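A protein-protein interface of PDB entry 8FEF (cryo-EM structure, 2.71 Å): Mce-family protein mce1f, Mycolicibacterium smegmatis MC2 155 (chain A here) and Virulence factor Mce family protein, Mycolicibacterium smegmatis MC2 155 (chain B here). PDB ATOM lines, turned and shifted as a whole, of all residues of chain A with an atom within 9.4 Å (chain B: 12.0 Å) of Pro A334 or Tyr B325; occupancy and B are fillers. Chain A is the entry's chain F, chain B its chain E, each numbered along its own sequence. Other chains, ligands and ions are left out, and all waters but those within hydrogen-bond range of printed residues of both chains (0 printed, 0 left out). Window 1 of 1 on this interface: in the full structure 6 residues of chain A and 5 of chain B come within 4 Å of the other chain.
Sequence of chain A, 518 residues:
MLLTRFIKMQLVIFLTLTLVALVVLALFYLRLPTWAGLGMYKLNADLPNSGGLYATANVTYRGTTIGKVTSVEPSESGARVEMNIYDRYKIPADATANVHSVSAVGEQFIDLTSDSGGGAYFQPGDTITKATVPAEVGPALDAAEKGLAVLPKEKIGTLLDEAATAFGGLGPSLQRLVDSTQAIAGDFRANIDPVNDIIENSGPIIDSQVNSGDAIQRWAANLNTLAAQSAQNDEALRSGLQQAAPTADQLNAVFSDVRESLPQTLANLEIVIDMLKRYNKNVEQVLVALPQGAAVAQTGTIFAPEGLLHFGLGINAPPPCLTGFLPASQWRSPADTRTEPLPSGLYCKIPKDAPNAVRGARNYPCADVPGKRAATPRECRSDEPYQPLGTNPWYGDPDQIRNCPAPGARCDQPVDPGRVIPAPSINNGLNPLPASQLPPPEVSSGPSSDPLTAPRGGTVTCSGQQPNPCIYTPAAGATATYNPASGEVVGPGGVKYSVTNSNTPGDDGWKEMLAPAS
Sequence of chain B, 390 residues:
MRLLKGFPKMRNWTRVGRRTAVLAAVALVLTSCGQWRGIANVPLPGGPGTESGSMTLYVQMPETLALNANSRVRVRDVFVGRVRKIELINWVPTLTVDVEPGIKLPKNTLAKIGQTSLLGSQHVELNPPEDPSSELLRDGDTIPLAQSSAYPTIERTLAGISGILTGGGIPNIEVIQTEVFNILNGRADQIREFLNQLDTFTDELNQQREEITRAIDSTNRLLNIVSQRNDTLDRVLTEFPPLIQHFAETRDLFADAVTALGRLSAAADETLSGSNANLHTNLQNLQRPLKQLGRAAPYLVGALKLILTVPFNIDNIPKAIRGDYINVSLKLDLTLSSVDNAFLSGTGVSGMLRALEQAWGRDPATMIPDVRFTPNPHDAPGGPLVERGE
The backbone carbonyl oxygen (O) of Lys B319 sits close to the guanidinium group (NH2) of Arg B322 (3.1 Å).
Of chain B, only Tyr B325 (3.5 Å) comes within 4 Å of Pro A334. Tyr B325 touches just these residues of chain A: Arg A332 and Pro A334. No residue of chain B comes within 4 Å of Trp A331. Thr A337 touches just one residue of chain B: Arg B322 (3.4 Å). No residue of chain A comes within 4 Å of Gly B323. Asp B324 touches just one residue of chain A: Arg A332. Of the printed residues of chain A, Arg B322 touches Asp A336 (3.99 Å) and Thr A337 (3.4 Å). Of the printed residues of chain B, Asp A336 touches Arg B322 (3.99 Å). Ala B320 touches none of the printed residues of chain A. The nearest residue of chain B that does not touch Pro A334 is Arg B322 (5.5 Å). The nearest printed residue of chain A that does not touch Arg B322 is Arg A338 (5.0 Å).
Among the printed residues, merely in contact across the chains: Thr A337 with Arg B322 (3.4 Å), Pro A334 with Tyr B325 (3.5 Å) and Asp A336 with Arg B322 (3.99 Å).
Of the 15 printed residues of chain B, 3 touch a printed residue of chain A. Of the 11 printed residues of chain A, 4 touch a printed residue of chain B. Hydrophobic or aromatic side chains of chain A that line the printed part of chain B: Pro A334. Among the printed residues, Asp or Glu carboxylates within 4 Å of a Lys or Arg side-chain nitrogen of the other chain: Arg A332 with Asp B324.
The side-chain carboxylate (OD2) of Asp B324 lies within salt-bridge range of the guanidinium group (NE) of Arg A332 (2.8 Å). The side-chain hydroxyl (OH) of Tyr B325 is in hydrogen-bond range of the backbone carbonyl oxygen (O) of Arg A332, 3.0 Å away.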
ATOM      1  N   LEU A 326      13.219 -14.889  23.360  1.00  0.00           N
ATOM      2  CA  LEU A 326      12.688 -13.711  22.694  1.00  0.00           C
ATOM      3  C   LEU A 326      11.167 -13.810  22.574  1.00  0.00           C
ATOM      4  O   LEU A 326      10.632 -14.898  22.348  1.00  0.00           O
ATOM      5  CB  LEU A 326      13.318 -13.566  21.309  1.00  0.00           C
ATOM      6  CG  LEU A 326      13.476 -12.166  20.722  1.00  0.00           C
ATOM      7  CD1 LEU A 326      14.337 -11.305  21.627  1.00  0.00           C
ATOM      8  CD2 LEU A 326      14.074 -12.249  19.330  1.00  0.00           C
ATOM      9  N   ALA A 328       7.327 -13.498  21.018  1.00  0.00           N
ATOM     10  CA  ALA A 328       6.806 -13.845  19.701  1.00  0.00           C
ATOM     11  C   ALA A 328       6.757 -12.630  18.783  1.00  0.00           C
ATOM     12  O   ALA A 328       7.083 -12.729  17.595  1.00  0.00           O
ATOM     13  CB  ALA A 328       5.418 -14.470  19.833  1.00  0.00           C
ATOM     14  N   GLN A 330       8.698 -10.223  18.641  1.00  0.00           N
ATOM     15  CA  GLN A 330      10.036  -9.798  18.253  1.00  0.00           C
ATOM     16  C   GLN A 330      10.686 -10.731  17.240  1.00  0.00           C
ATOM     17  O   GLN A 330      11.843 -10.506  16.870  1.00  0.00           O
ATOM     18  CB  GLN A 330      10.931  -9.676  19.490  1.00  0.00           C
ATOM     19  CG  GLN A 330      10.394  -8.734  20.557  1.00  0.00           C
ATOM     20  CD  GLN A 330      10.143  -7.334  20.033  1.00  0.00           C
ATOM     21  OE1 GLN A 330      11.073  -6.545  19.866  1.00  0.00           O
ATOM     22  NE2 GLN A 330       8.880  -7.016  19.775  1.00  0.00           N
ATOM     23  N   TRP A 331       9.981 -11.768  16.794  1.00  0.00           N
ATOM     24  CA  TRP A 331      10.512 -12.654  15.769  1.00  0.00           C
ATOM     25  C   TRP A 331      10.644 -11.911  14.443  1.00  0.00           C
ATOM     26  O   TRP A 331       9.879 -10.992  14.140  1.00  0.00           O
ATOM     27  CB  TRP A 331       9.612 -13.876  15.592  1.00  0.00           C
ATOM     28  CG  TRP A 331       9.689 -14.859  16.718  1.00  0.00           C
ATOM     29  CD1 TRP A 331      10.365 -14.710  17.892  1.00  0.00           C
ATOM     30  CD2 TRP A 331       9.065 -16.146  16.776  1.00  0.00           C
ATOM     31  NE1 TRP A 331      10.202 -15.824  18.678  1.00  0.00           N
ATOM     32  CE2 TRP A 331       9.407 -16.720  18.015  1.00  0.00           C
ATOM     33  CE3 TRP A 331       8.250 -16.868  15.900  1.00  0.00           C
ATOM     34  CZ2 TRP A 331       8.963 -17.982  18.400  1.00  0.00           C
ATOM     35  CZ3 TRP A 331       7.811 -18.119  16.283  1.00  0.00           C
ATOM     36  CH2 TRP A 331       8.167 -18.664  17.522  1.00  0.00           C
ATOM     37  N   ARG A 332      11.630 -12.318  13.652  1.00  0.00           N
ATOM     38  CA  ARG A 332      11.919 -11.679  12.377  1.00  0.00           C
ATOM     39  C   ARG A 332      11.409 -12.537  11.229  1.00  0.00           C
ATOM     40  O   ARG A 332      11.466 -13.768  11.284  1.00  0.00           O
ATOM     41  CB  ARG A 332      13.420 -11.428  12.225  1.00  0.00           C
ATOM     42  CG  ARG A 332      14.138 -11.237  13.550  1.00  0.00           C
ATOM     43  CD  ARG A 332      15.394 -10.391  13.419  1.00  0.00           C
ATOM     44  NE  ARG A 332      16.357 -10.950  12.480  1.00  0.00           N
ATOM     45  CZ  ARG A 332      16.661 -10.410  11.308  1.00  0.00           C
ATOM     46  NH1 ARG A 332      16.104  -9.281  10.903  1.00  0.00           N
ATOM     47  NH2 ARG A 332      17.546 -11.016  10.526  1.00  0.00           N
ATOM     48  N   SER A 333      10.893 -11.873  10.199  1.00  0.00           N
ATOM     49  CA  SER A 333      10.372 -12.575   9.037  1.00  0.00           C
ATOM     50  C   SER A 333      11.496 -13.339   8.342  1.00  0.00           C
ATOM     51  O   SER A 333      12.634 -12.858   8.295  1.00  0.00           O
ATOM     52  CB  SER A 333       9.724 -11.585   8.068  1.00  0.00           C
ATOM     53  OG  SER A 333       9.123 -12.248   6.972  1.00  0.00           O
ATOM     54  N   PRO A 334      11.224 -14.535   7.812  1.00  0.00           N
ATOM     55  CA  PRO A 334      12.302 -15.327   7.194  1.00  0.00           C
ATOM     56  C   PRO A 334      12.916 -14.682   5.963  1.00  0.00           C
ATOM     57  O   PRO A 334      14.019 -15.075   5.566  1.00  0.00           O
ATOM     58  CB  PRO A 334      11.611 -16.653   6.849  1.00  0.00           C
ATOM     59  CG  PRO A 334      10.158 -16.318   6.773  1.00  0.00           C
ATOM     60  CD  PRO A 334       9.934 -15.244   7.791  1.00  0.00           C
ATOM     61  N   ALA A 335      12.238 -13.711   5.348  1.00  0.00           N
ATOM     62  CA  ALA A 335      12.783 -13.057   4.163  1.00  0.00           C
ATOM     63  C   ALA A 335      14.005 -12.215   4.503  1.00  0.00           C
ATOM     64  O   ALA A 335      14.951 -12.138   3.711  1.00  0.00           O
ATOM     65  CB  ALA A 335      11.709 -12.196   3.500  1.00  0.00           C
ATOM     66  N   ASP A 336      14.003 -11.571   5.669  1.00  0.00           N
ATOM     67  CA  ASP A 336      15.089 -10.674   6.055  1.00  0.00           C
ATOM     68  C   ASP A 336      16.348 -11.482   6.343  1.00  0.00           C
ATOM     69  O   ASP A 336      16.450 -12.135   7.386  1.00  0.00           O
ATOM     70  CB  ASP A 336      14.683  -9.849   7.272  1.00  0.00           C
ATOM     71  CG  ASP A 336      13.513  -8.926   6.988  1.00  0.00           C
ATOM     72  OD1 ASP A 336      13.385  -8.461   5.837  1.00  0.00           O
ATOM     73  OD2 ASP A 336      12.721  -8.665   7.916  1.00  0.00           O
ATOM     74  N   THR A 337      17.307 -11.437   5.421  1.00  0.00           N
ATOM     75  CA  THR A 337      18.602 -12.078   5.607  1.00  0.00           C
ATOM     76  C   THR A 337      19.584 -11.203   6.374  1.00  0.00           C
ATOM     77  O   THR A 337      20.716 -11.633   6.616  1.00  0.00           O
ATOM     78  CB  THR A 337      19.204 -12.455   4.251  1.00  0.00           C
ATOM     79  OG1 THR A 337      19.383 -11.274   3.462  1.00  0.00           O
ATOM     80  CG2 THR A 337      18.288 -13.414   3.513  1.00  0.00           C
ATOM     81  N   ARG A 338      19.177  -9.994   6.746  1.00  0.00           N
ATOM     82  CA  ARG A 338      20.036  -9.085   7.488  1.00  0.00           C
ATOM     83  C   ARG A 338      20.350  -9.642   8.871  1.00  0.00           C
ATOM     84  O   ARG A 338      19.510 -10.282   9.507  1.00  0.00           O
ATOM     85  CB  ARG A 338      19.351  -7.723   7.602  1.00  0.00           C
ATOM     86  CG  ARG A 338      20.162  -6.628   8.258  1.00  0.00           C
ATOM     87  CD  ARG A 338      19.486  -5.292   8.020  1.00  0.00           C
ATOM     88  NE  ARG A 338      18.045  -5.384   8.225  1.00  0.00           N
ATOM     89  CZ  ARG A 338      17.159  -4.544   7.707  1.00  0.00           C
ATOM     90  NH1 ARG A 338      17.529  -3.540   6.930  1.00  0.00           N
ATOM     91  NH2 ARG A 338      15.867  -4.719   7.974  1.00  0.00           N
ATOM     92  N   PHE B 312      29.213 -27.518  12.312  1.00  0.00           N
ATOM     93  CA  PHE B 312      29.330 -26.415  11.374  1.00  0.00           C
ATOM     94  C   PHE B 312      30.779 -26.263  10.933  1.00  0.00           C
ATOM     95  O   PHE B 312      31.712 -26.513  11.701  1.00  0.00           O
ATOM     96  CB  PHE B 312      28.847 -25.108  12.006  1.00  0.00           C
ATOM     97  CG  PHE B 312      27.401 -25.121  12.410  1.00  0.00           C
ATOM     98  CD1 PHE B 312      26.996 -25.729  13.587  1.00  0.00           C
ATOM     99  CD2 PHE B 312      26.447 -24.507  11.619  1.00  0.00           C
ATOM    100  CE1 PHE B 312      25.669 -25.737  13.957  1.00  0.00           C
ATOM    101  CE2 PHE B 312      25.119 -24.509  11.986  1.00  0.00           C
ATOM    102  CZ  PHE B 312      24.729 -25.124  13.157  1.00  0.00           C
ATOM    103  N   ASN B 316      31.713 -21.935   5.157  1.00  0.00           N
ATOM    104  CA  ASN B 316      30.488 -21.737   4.390  1.00  0.00           C
ATOM    105  C   ASN B 316      29.296 -21.334   5.256  1.00  0.00           C
ATOM    106  O   ASN B 316      28.151 -21.422   4.802  1.00  0.00           O
ATOM    107  CB  ASN B 316      30.164 -22.995   3.586  1.00  0.00           C
ATOM    108  CG  ASN B 316      31.273 -23.376   2.625  1.00  0.00           C
ATOM    109  OD1 ASN B 316      31.937 -22.511   2.051  1.00  0.00           O
ATOM    110  ND2 ASN B 316      31.481 -24.675   2.444  1.00  0.00           N
ATOM    111  N   ILE B 317      29.537 -20.905   6.497  1.00  0.00           N
ATOM    112  CA  ILE B 317      28.440 -20.423   7.344  1.00  0.00           C
ATOM    113  C   ILE B 317      27.731 -19.199   6.765  1.00  0.00           C
ATOM    114  O   ILE B 317      26.489 -19.178   6.773  1.00  0.00           O
ATOM    115  CB  ILE B 317      28.944 -20.190   8.780  1.00  0.00           C
ATOM    116  CG1 ILE B 317      29.192 -21.526   9.478  1.00  0.00           C
ATOM    117  CG2 ILE B 317      27.947 -19.367   9.577  1.00  0.00           C
ATOM    118  CD1 ILE B 317      29.610 -21.392  10.922  1.00  0.00           C
ATOM    119  N   PRO B 318      28.424 -18.161   6.263  1.00  0.00           N
ATOM    120  CA  PRO B 318      27.701 -16.932   5.881  1.00  0.00           C
ATOM    121  C   PRO B 318      26.652 -17.116   4.794  1.00  0.00           C
ATOM    122  O   PRO B 318      25.748 -16.278   4.691  1.00  0.00           O
ATOM    123  CB  PRO B 318      28.823 -15.997   5.411  1.00  0.00           C
ATOM    124  CG  PRO B 318      30.007 -16.454   6.136  1.00  0.00           C
ATOM    125  CD  PRO B 318      29.882 -17.940   6.195  1.00  0.00           C
ATOM    126  N   LYS B 319      26.737 -18.168   3.980  1.00  0.00           N
ATOM    127  CA  LYS B 319      25.760 -18.378   2.919  1.00  0.00           C
ATOM    128  C   LYS B 319      24.692 -19.400   3.278  1.00  0.00           C
ATOM    129  O   LYS B 319      23.547 -19.254   2.840  1.00  0.00           O
ATOM    130  CB  LYS B 319      26.456 -18.810   1.624  1.00  0.00           C
ATOM    131  CG  LYS B 319      27.423 -19.971   1.766  1.00  0.00           C
ATOM    132  CD  LYS B 319      28.138 -20.221   0.449  1.00  0.00           C
ATOM    133  CE  LYS B 319      29.218 -21.276   0.577  1.00  0.00           C
ATOM    134  NZ  LYS B 319      29.956 -21.462  -0.704  1.00  0.00           N
ATOM    135  N   ALA B 320      25.033 -20.430   4.052  1.00  0.00           N
ATOM    136  CA  ALA B 320      24.029 -21.408   4.460  1.00  0.00           C
ATOM    137  C   ALA B 320      23.051 -20.813   5.465  1.00  0.00           C
ATOM    138  O   ALA B 320      21.839 -21.025   5.359  1.00  0.00           O
ATOM    139  CB  ALA B 320      24.708 -22.647   5.042  1.00  0.00           C
ATOM    140  N   ILE B 321      23.556 -20.065   6.442  1.00  0.00           N
ATOM    141  CA  ILE B 321      22.737 -19.459   7.485  1.00  0.00           C
ATOM    142  C   ILE B 321      22.515 -18.000   7.113  1.00  0.00           C
ATOM    143  O   ILE B 321      23.422 -17.172   7.247  1.00  0.00           O
ATOM    144  CB  ILE B 321      23.398 -19.584   8.865  1.00  0.00           C
ATOM    145  CG1 ILE B 321      23.801 -21.033   9.136  1.00  0.00           C
ATOM    146  CG2 ILE B 321      22.457 -19.098   9.947  1.00  0.00           C
ATOM    147  CD1 ILE B 321      24.451 -21.238  10.480  1.00  0.00           C
ATOM    148  N   ARG B 322      21.314 -17.674   6.648  1.00  0.00           N
ATOM    149  CA  ARG B 322      20.989 -16.300   6.261  1.00  0.00           C
ATOM    150  C   ARG B 322      20.359 -15.533   7.418  1.00  0.00           C
ATOM    151  O   ARG B 322      19.283 -14.947   7.304  1.00  0.00           O
ATOM    152  CB  ARG B 322      20.073 -16.298   5.043  1.00  0.00           C
ATOM    153  CG  ARG B 322      20.605 -17.080   3.864  1.00  0.00           C
ATOM    154  CD  ARG B 322      21.885 -16.478   3.331  1.00  0.00           C
ATOM    155  NE  ARG B 322      22.454 -17.294   2.268  1.00  0.00           N
ATOM    156  CZ  ARG B 322      22.162 -17.157   0.983  1.00  0.00           C
ATOM    157  NH1 ARG B 322      21.323 -16.227   0.561  1.00  0.00           N
ATOM    158  NH2 ARG B 322      22.727 -17.974   0.100  1.00  0.00           N
ATOM    159  N   GLY B 323      21.047 -15.533   8.554  1.00  0.00           N
ATOM    160  CA  GLY B 323      20.583 -14.814   9.722  1.00  0.00           C
ATOM    161  C   GLY B 323      19.839 -15.677  10.718  1.00  0.00           C
ATOM    162  O   GLY B 323      20.452 -16.460  11.449  1.00  0.00           O
ATOM    163  N   ASP B 324      18.512 -15.542  10.755  1.00  0.00           N
ATOM    164  CA  ASP B 324      17.730 -16.228  11.778  1.00  0.00           C
ATOM    165  C   ASP B 324      17.616 -17.722  11.499  1.00  0.00           C
ATOM    166  O   ASP B 324      17.727 -18.537  12.420  1.00  0.00           O
ATOM    167  CB  ASP B 324      16.339 -15.608  11.871  1.00  0.00           C
ATOM    168  CG  ASP B 324      16.384 -14.117  12.089  1.00  0.00           C
ATOM    169  OD1 ASP B 324      16.961 -13.676  13.104  1.00  0.00           O
ATOM    170  OD2 ASP B 324      15.853 -13.384  11.231  1.00  0.00           O
ATOM    171  N   TYR B 325      17.396 -18.100  10.245  1.00  0.00           N
ATOM    172  CA  TYR B 325      17.020 -19.462   9.890  1.00  0.00           C
ATOM    173  C   TYR B 325      18.110 -20.123   9.059  1.00  0.00           C
ATOM    174  O   TYR B 325      18.593 -19.540   8.084  1.00  0.00           O
ATOM    175  CB  TYR B 325      15.696 -19.477   9.125  1.00  0.00           C
ATOM    176  CG  TYR B 325      14.576 -18.732   9.813  1.00  0.00           C
ATOM    177  CD1 TYR B 325      14.365 -17.384   9.580  1.00  0.00           C
ATOM    178  CD2 TYR B 325      13.724 -19.381  10.691  1.00  0.00           C
ATOM    179  CE1 TYR B 325      13.347 -16.704  10.207  1.00  0.00           C
ATOM    180  CE2 TYR B 325      12.699 -18.708  11.320  1.00  0.00           C
ATOM    181  CZ  TYR B 325      12.513 -17.370  11.073  1.00  0.00           C
ATOM    182  OH  TYR B 325      11.493 -16.690  11.698  1.00  0.00           O
ATOM    183  N   ILE B 326      18.482 -21.340   9.443  1.00  0.00           N
ATOM    184  CA  ILE B 326      19.436 -22.131   8.676  1.00  0.00           C
ATOM    185  C   ILE B 326      18.730 -22.700   7.454  1.00  0.00           C
ATOM    186  O   ILE B 326      17.648 -23.288   7.566  1.00  0.00           O
ATOM    187  CB  ILE B 326      20.027 -23.258   9.539  1.00  0.00           C
ATOM    188  CG1 ILE B 326      20.614 -22.698  10.832  1.00  0.00           C
ATOM    189  CG2 ILE B 326      21.081 -24.021   8.762  1.00  0.00           C
ATOM    190  CD1 ILE B 326      21.143 -23.759  11.769  1.00  0.00           C
ATOM    191  N   ASN B 327      19.334 -22.524   6.283  1.00  0.00           N
ATOM    192  CA  ASN B 327      18.828 -23.156   5.072  1.00  0.00           C
ATOM    193  C   ASN B 327      19.174 -24.638   5.074  1.00  0.00           C
ATOM    194  O   ASN B 327      20.247 -25.040   5.533  1.00  0.00           O
ATOM    195  CB  ASN B 327      19.408 -22.485   3.830  1.00  0.00           C
ATOM    196  CG  ASN B 327      18.807 -21.123   3.570  1.00  0.00           C
ATOM    197  OD1 ASN B 327      18.002 -20.625   4.353  1.00  0.00           O
ATOM    198  ND2 ASN B 327      19.205 -20.506   2.468  1.00  0.00           N
ATOM    199  N   VAL B 328      18.270 -25.455   4.556  1.00  0.00           N
ATOM    200  CA  VAL B 328      18.498 -26.886   4.522  1.00  0.00           C
ATOM    201  C   VAL B 328      17.686 -27.517   3.404  1.00  0.00           C
ATOM    202  O   VAL B 328      16.606 -27.038   3.065  1.00  0.00           O
ATOM    203  CB  VAL B 328      18.115 -27.530   5.863  1.00  0.00           C
ATOM    204  CG1 VAL B 328      16.606 -27.637   5.987  1.00  0.00           C
ATOM    205  CG2 VAL B 328      18.769 -28.893   6.011  1.00  0.00           C
ATOM    206  N   SER B 329      18.216 -28.586   2.824  1.00  0.00           N
ATOM    207  CA  SER B 329      17.526 -29.284   1.753  1.00  0.00           C
ATOM    208  C   SER B 329      16.974 -30.577   2.325  1.00  0.00           C
ATOM    209  O   SER B 329      17.724 -31.429   2.797  1.00  0.00           O
ATOM    210  CB  SER B 329      18.488 -29.581   0.603  1.00  0.00           C
ATOM    211  OG  SER B 329      18.960 -28.381   0.019  1.00  0.00           O
